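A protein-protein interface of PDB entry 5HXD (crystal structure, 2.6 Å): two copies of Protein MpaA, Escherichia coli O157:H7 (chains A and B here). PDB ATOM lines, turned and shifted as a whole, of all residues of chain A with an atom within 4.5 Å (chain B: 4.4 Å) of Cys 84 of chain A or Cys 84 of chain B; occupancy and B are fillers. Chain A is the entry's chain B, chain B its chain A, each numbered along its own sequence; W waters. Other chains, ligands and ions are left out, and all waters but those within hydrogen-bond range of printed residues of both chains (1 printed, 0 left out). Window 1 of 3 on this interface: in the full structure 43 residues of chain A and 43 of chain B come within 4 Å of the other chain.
O of Cys 84 of chain B lies within hydrogen-bond range of SG of Cys 84 of chain A.
Water W1 bridges O of Cys 78 of chain B and OE1 of Gln 85 of chain A.
Among the printed residues, pairs that only touch across the chains: Cys 78 of chain A with Gln 85 of chain B (3.2 Å), Pro 81 of chain A with Gln 85 of chain B (3.3 Å), Gln 85 of chain A with Cys 78 of chain B (3.2 Å) and Gln 85 of chain A with Pro 81 of chain B (3.3 Å).
Hydrophobic or aromatic side chains of chain A that line the printed part of chain B: Pro 81. Of the 10 printed residues of chain B, 4 touch a printed residue of chain A. Hydrophobic or aromatic side chains of chain B within 4 Å of the printed part of chain A: Pro 81. Among the printed residues, no Asp or Glu carboxylate lies within 4 Å of a Lys or Arg side-chain nitrogen of the other chain.
SG of Cys 78 of chain A sits at hydrogen-bond distance from O of Asn 80 of chain A, 3.3 Å away. The side-chain amide nitrogen (ND2) of Asn 53 of chain A lies within hydrogen-bond range of the side-chain sulfur (SG) of Cys 84 of chain A (3.6 Å). The side-chain sulfur (SG) of Cys 84 of chain B forms a disulfide with the side-chain sulfur (SG) of Cys 78 of chain B.
Cys 78 of chain A touches Gln 85 of chain B, and with the chains exchanged Gln 85 of chain A touches Cys 78 of chain B. Pro 81 of chain A touches Gln 85 of chain B, and with the chains exchanged Gln 85 of chain A touches Pro 81 of chain B. Cys 84 of chain A touches its own counterpart, Cys 84 of chain B. Positions printed for both chains: 50, 78, 80, 81, 82, 83, 84, 85, 86 and 87. Of the 5 pairs that touch across the chains among the printed residues, 5 have their exchanged pair printed and touching as well.
Cys 84 of chain A touches one residue of chain B. Of chain A, only Cys 84 comes within 4 Å of Cys 84 of chain B. Of the printed residues of chain B, Pro 81 of chain A touches Gln 85 (3.3 Å). Of the printed residues of chain A, Gln 85 of chain B touches Cys 78 and Pro 81. Printed residues of chain A within 4 Å of Cys 78 of chain B: Gln 85. Printed residues of chain B within 4 Å of Gln 85 of chain A: Cys 78 and Pro 81. Of the printed residues of chain B, Cys 78 of chain A touches Gln 85. Leu 86 of chain A touches none of the printed residues of chain B. Gly 50 of chain A touches none of the printed residues of chain B. The nearest residue of chain B that does not touch Cys 84 of chain A is Gln 85 of chain B (4.2 Å). The nearest residue of chain A that does not touch Cys 84 of chain B is Val 56 of chain A (4.2 Å).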
ATOM      1  N   GLY A  50      16.635  11.434 -16.855  1.00  0.00           N
ATOM      2  CA  GLY A  50      15.720  10.659 -16.021  1.00  0.00           C
ATOM      3  C   GLY A  50      14.570  11.434 -15.390  1.00  0.00           C
ATOM      4  O   GLY A  50      13.526  10.860 -15.094  1.00  0.00           O
ATOM      5  N   ASN A  53       9.965  13.529 -17.730  1.00  0.00           N
ATOM      6  CA  ASN A  53       9.076  12.376 -17.794  1.00  0.00           C
ATOM      7  C   ASN A  53       7.717  12.653 -18.399  1.00  0.00           C
ATOM      8  O   ASN A  53       6.941  11.731 -18.646  1.00  0.00           O
ATOM      9  CB  ASN A  53       8.844  11.848 -16.395  1.00  0.00           C
ATOM     10  CG  ASN A  53      10.113  11.463 -15.669  1.00  0.00           C
ATOM     11  OD1 ASN A  53      10.468  12.082 -14.657  1.00  0.00           O
ATOM     12  ND2 ASN A  53      10.784  10.411 -16.149  1.00  0.00           N
ATOM     13  N   VAL A  56       8.164  11.355 -21.727  1.00  0.00           N
ATOM     14  CA  VAL A  56       8.186   9.877 -21.702  1.00  0.00           C
ATOM     15  C   VAL A  56       6.773   9.296 -21.652  1.00  0.00           C
ATOM     16  O   VAL A  56       6.408   8.427 -22.457  1.00  0.00           O
ATOM     17  CB  VAL A  56       8.981   9.302 -20.487  1.00  0.00           C
ATOM     18  CG1 VAL A  56       8.890   7.783 -20.437  1.00  0.00           C
ATOM     19  CG2 VAL A  56      10.449   9.727 -20.518  1.00  0.00           C
ATOM     20  N   CYS A  78      12.617   5.733 -23.316  1.00  0.00           N
ATOM     21  CA  CYS A  78      13.507   6.114 -22.249  1.00  0.00           C
ATOM     22  C   CYS A  78      14.936   5.715 -22.563  1.00  0.00           C
ATOM     23  O   CYS A  78      15.266   4.527 -22.589  1.00  0.00           O
ATOM     24  CB  CYS A  78      13.062   5.479 -20.924  1.00  0.00           C
ATOM     25  SG  CYS A  78      14.049   6.045 -19.541  1.00  0.00           S
ATOM     26  N   ASN A  80      17.460   6.602 -20.721  1.00  0.00           N
ATOM     27  CA  ASN A  80      18.165   6.527 -19.451  1.00  0.00           C
ATOM     28  C   ASN A  80      17.240   5.941 -18.382  1.00  0.00           C
ATOM     29  O   ASN A  80      16.654   6.677 -17.602  1.00  0.00           O
ATOM     30  CB  ASN A  80      18.666   7.935 -19.094  1.00  0.00           C
ATOM     31  CG  ASN A  80      19.321   8.022 -17.728  1.00  0.00           C
ATOM     32  OD1 ASN A  80      19.718   7.017 -17.141  1.00  0.00           O
ATOM     33  ND2 ASN A  80      19.458   9.240 -17.232  1.00  0.00           N
ATOM     34  N   PRO A  81      17.104   4.604 -18.352  1.00  0.00           N
ATOM     35  CA  PRO A  81      16.109   3.947 -17.492  1.00  0.00           C
ATOM     36  C   PRO A  81      16.550   3.832 -16.011  1.00  0.00           C
ATOM     37  O   PRO A  81      15.719   3.772 -15.096  1.00  0.00           O
ATOM     38  CB  PRO A  81      15.953   2.572 -18.149  1.00  0.00           C
ATOM     39  CG  PRO A  81      17.265   2.309 -18.786  1.00  0.00           C
ATOM     40  CD  PRO A  81      17.958   3.624 -19.043  1.00  0.00           C
ATOM     41  N   ASP A  82      17.853   3.816 -15.774  1.00  0.00           N
ATOM     42  CA  ASP A  82      18.337   3.862 -14.415  1.00  0.00           C
ATOM     43  C   ASP A  82      18.004   5.243 -13.852  1.00  0.00           C
ATOM     44  O   ASP A  82      17.214   5.341 -12.913  1.00  0.00           O
ATOM     45  CB  ASP A  82      19.840   3.541 -14.333  1.00  0.00           C
ATOM     46  CG  ASP A  82      20.165   2.092 -14.780  1.00  0.00           C
ATOM     47  OD1 ASP A  82      19.231   1.246 -14.871  1.00  0.00           O
ATOM     48  OD2 ASP A  82      21.355   1.796 -15.047  1.00  0.00           O
ATOM     49  N   GLY A  83      18.560   6.305 -14.432  1.00  0.00           N
ATOM     50  CA  GLY A  83      18.239   7.660 -14.001  1.00  0.00           C
ATOM     51  C   GLY A  83      16.734   7.838 -13.858  1.00  0.00           C
ATOM     52  O   GLY A  83      16.238   8.550 -12.975  1.00  0.00           O
ATOM     53  N   CYS A  84      15.986   7.141 -14.710  1.00  0.00           N
ATOM     54  CA  CYS A  84      14.538   7.272 -14.692  1.00  0.00           C
ATOM     55  C   CYS A  84      13.898   6.677 -13.425  1.00  0.00           C
ATOM     56  O   CYS A  84      13.041   7.332 -12.838  1.00  0.00           O
ATOM     57  CB  CYS A  84      13.909   6.650 -15.946  1.00  0.00           C
ATOM     58  SG  CYS A  84      12.138   7.088 -16.110  1.00  0.00           S
ATOM     59  N   GLN A  85      14.275   5.465 -12.998  1.00  0.00           N
ATOM     60  CA  GLN A  85      13.699   4.939 -11.731  1.00  0.00           C
ATOM     61  C   GLN A  85      14.270   5.630 -10.496  1.00  0.00           C
ATOM     62  O   GLN A  85      13.640   5.619  -9.444  1.00  0.00           O
ATOM     63  CB  GLN A  85      13.871   3.416 -11.571  1.00  0.00           C
ATOM     64  CG  GLN A  85      15.293   2.906 -11.484  1.00  0.00           C
ATOM     65  CD  GLN A  85      15.349   1.563 -10.802  1.00  0.00           C
ATOM     66  OE1 GLN A  85      14.732   1.383  -9.759  1.00  0.00           O
ATOM     67  NE2 GLN A  85      16.059   0.611 -11.379  1.00  0.00           N
ATOM     68  N   LEU A  86      15.452   6.230 -10.635  1.00  0.00           N
ATOM     69  CA  LEU A  86      16.073   7.000  -9.557  1.00  0.00           C
ATOM     70  C   LEU A  86      15.595   8.440  -9.527  1.00  0.00           C
ATOM     71  O   LEU A  86      16.170   9.272  -8.827  1.00  0.00           O
ATOM     72  CB  LEU A  86      17.588   6.984  -9.693  1.00  0.00           C
ATOM     73  CG  LEU A  86      18.206   5.612  -9.448  1.00  0.00           C
ATOM     74  CD1 LEU A  86      19.621   5.594  -9.996  1.00  0.00           C
ATOM     75  CD2 LEU A  86      18.162   5.230  -7.952  1.00  0.00           C
ATOM     76  N   GLY A  87      14.541   8.720 -10.287  1.00  0.00           N
ATOM     77  CA  GLY A  87      14.063  10.074 -10.494  1.00  0.00           C
ATOM     78  C   GLY A  87      15.129  11.145 -10.652  1.00  0.00           C
ATOM     79  O   GLY A  87      14.911  12.266 -10.210  1.00  0.00           O
ATOM     80  N   LEU A  88      16.282  10.833 -11.245  1.00  0.00           N
ATOM     81  CA  LEU A  88      17.272  11.893 -11.471  1.00  0.00           C
ATOM     82  C   LEU A  88      17.777  12.037 -12.891  1.00  0.00           C
ATOM     83  O   LEU A  88      17.763  11.098 -13.683  1.00  0.00           O
ATOM     84  CB  LEU A  88      18.503  11.745 -10.566  1.00  0.00           C
ATOM     85  CG  LEU A  88      19.517  10.608 -10.423  1.00  0.00           C
ATOM     86  CD1 LEU A  88      20.388  10.397 -11.585  1.00  0.00           C
ATOM     87  CD2 LEU A  88      20.406  10.996  -9.247  1.00  0.00           C
ATOM     88  N   GLY B  50       4.126   3.356 -12.764  1.00  0.00           N
ATOM     89  CA  GLY B  50       5.229   3.945 -13.515  1.00  0.00           C
ATOM     90  C   GLY B  50       5.028   5.290 -14.204  1.00  0.00           C
ATOM     91  O   GLY B  50       6.004   5.953 -14.527  1.00  0.00           O
ATOM     92  N   CYS B  78      11.282   3.931  -6.381  1.00  0.00           N
ATOM     93  CA  CYS B  78      10.508   3.378  -7.480  1.00  0.00           C
ATOM     94  C   CYS B  78      10.186   1.889  -7.289  1.00  0.00           C
ATOM     95  O   CYS B  78      11.041   1.011  -7.462  1.00  0.00           O
ATOM     96  CB  CYS B  78      11.257   3.616  -8.796  1.00  0.00           C
ATOM     97  SG  CYS B  78      10.264   3.432 -10.266  1.00  0.00           S
ATOM     98  N   ASN B  80       8.197   0.216  -9.131  1.00  0.00           N
ATOM     99  CA  ASN B  80       7.966  -0.362 -10.457  1.00  0.00           C
ATOM    100  C   ASN B  80       8.895   0.208 -11.521  1.00  0.00           C
ATOM    101  O   ASN B  80       8.446   0.893 -12.413  1.00  0.00           O
ATOM    102  CB  ASN B  80       6.503  -0.113 -10.832  1.00  0.00           C
ATOM    103  CG  ASN B  80       6.106  -0.691 -12.173  1.00  0.00           C
ATOM    104  OD1 ASN B  80       6.819  -1.502 -12.761  1.00  0.00           O
ATOM    105  ND2 ASN B  80       4.937  -0.286 -12.655  1.00  0.00           N
ATOM    106  N   PRO B  81      10.202  -0.077 -11.438  1.00  0.00           N
ATOM    107  CA  PRO B  81      11.163   0.576 -12.342  1.00  0.00           C
ATOM    108  C   PRO B  81      11.011   0.235 -13.833  1.00  0.00           C
ATOM    109  O   PRO B  81      11.556   0.974 -14.673  1.00  0.00           O
ATOM    110  CB  PRO B  81      12.523   0.093 -11.819  1.00  0.00           C
ATOM    111  CG  PRO B  81      12.244  -1.081 -10.983  1.00  0.00           C
ATOM    112  CD  PRO B  81      10.865  -0.940 -10.450  1.00  0.00           C
ATOM    113  N   ASP B  82      10.307  -0.853 -14.155  1.00  0.00           N
ATOM    114  CA  ASP B  82       9.962  -1.169 -15.554  1.00  0.00           C
ATOM    115  C   ASP B  82       8.780  -0.307 -16.008  1.00  0.00           C
ATOM    116  O   ASP B  82       8.694   0.077 -17.168  1.00  0.00           O
ATOM    117  CB  ASP B  82       9.605  -2.656 -15.745  1.00  0.00           C
ATOM    118  CG  ASP B  82      10.780  -3.588 -15.532  1.00  0.00           C
ATOM    119  OD1 ASP B  82      11.944  -3.134 -15.513  1.00  0.00           O
ATOM    120  OD2 ASP B  82      10.525  -4.799 -15.392  1.00  0.00           O
ATOM    121  N   GLY B  83       7.860  -0.047 -15.080  1.00  0.00           N
ATOM    122  CA  GLY B  83       6.772   0.890 -15.292  1.00  0.00           C
ATOM    123  C   GLY B  83       7.290   2.276 -15.645  1.00  0.00           C
ATOM    124  O   GLY B  83       6.980   2.767 -16.742  1.00  0.00           O
ATOM    125  N   CYS B  84       8.074   2.890 -14.739  1.00  0.00           N
ATOM    126  CA  CYS B  84       8.616   4.244 -14.931  1.00  0.00           C
ATOM    127  C   CYS B  84       9.324   4.390 -16.315  1.00  0.00           C
ATOM    128  O   CYS B  84       9.127   5.389 -17.016  1.00  0.00           O
ATOM    129  CB  CYS B  84       9.614   4.655 -13.811  1.00  0.00           C
ATOM    130  SG  CYS B  84       9.541   3.874 -12.162  1.00  0.00           S
ATOM    131  N   GLN B  85      10.147   3.407 -16.687  1.00  0.00           N
ATOM    132  CA  GLN B  85      10.921   3.464 -17.938  1.00  0.00           C
ATOM    133  C   GLN B  85      10.016   3.405 -19.170  1.00  0.00           C
ATOM    134  O   GLN B  85      10.305   4.027 -20.193  1.00  0.00           O
ATOM    135  CB  GLN B  85      11.975   2.337 -17.978  1.00  0.00           C
ATOM    136  CG  GLN B  85      11.931   1.524 -19.222  1.00  0.00           C
ATOM    137  CD  GLN B  85      13.214   0.803 -19.541  1.00  0.00           C
ATOM    138  OE1 GLN B  85      13.773   0.095 -18.724  1.00  0.00           O
ATOM    139  NE2 GLN B  85      13.690   0.990 -20.764  1.00  0.00           N
ATOM    140  N   LEU B  86       8.913   2.670 -19.043  1.00  0.00           N
ATOM    141  CA  LEU B  86       7.924   2.525 -20.101  1.00  0.00           C
ATOM    142  C   LEU B  86       6.797   3.574 -20.037  1.00  0.00           C
ATOM    143  O   LEU B  86       5.845   3.476 -20.803  1.00  0.00           O
ATOM    144  CB  LEU B  86       7.308   1.115 -20.059  1.00  0.00           C
ATOM    145  CG  LEU B  86       8.200  -0.094 -20.362  1.00  0.00           C
ATOM    146  CD1 LEU B  86       7.538  -1.403 -19.937  1.00  0.00           C
ATOM    147  CD2 LEU B  86       8.555  -0.127 -21.860  1.00  0.00           C
ATOM    148  N   GLY B  87       6.886   4.557 -19.135  1.00  0.00           N
ATOM    149  CA  GLY B  87       5.843   5.574 -19.002  1.00  0.00           C
ATOM    150  C   GLY B  87       4.442   4.997 -18.832  1.00  0.00           C
ATOM    151  O   GLY B  87       3.420   5.634 -19.111  1.00  0.00           O
HETATM  152  O   HOH W   1      13.378   0.043  -7.534  1.00  0.00           O
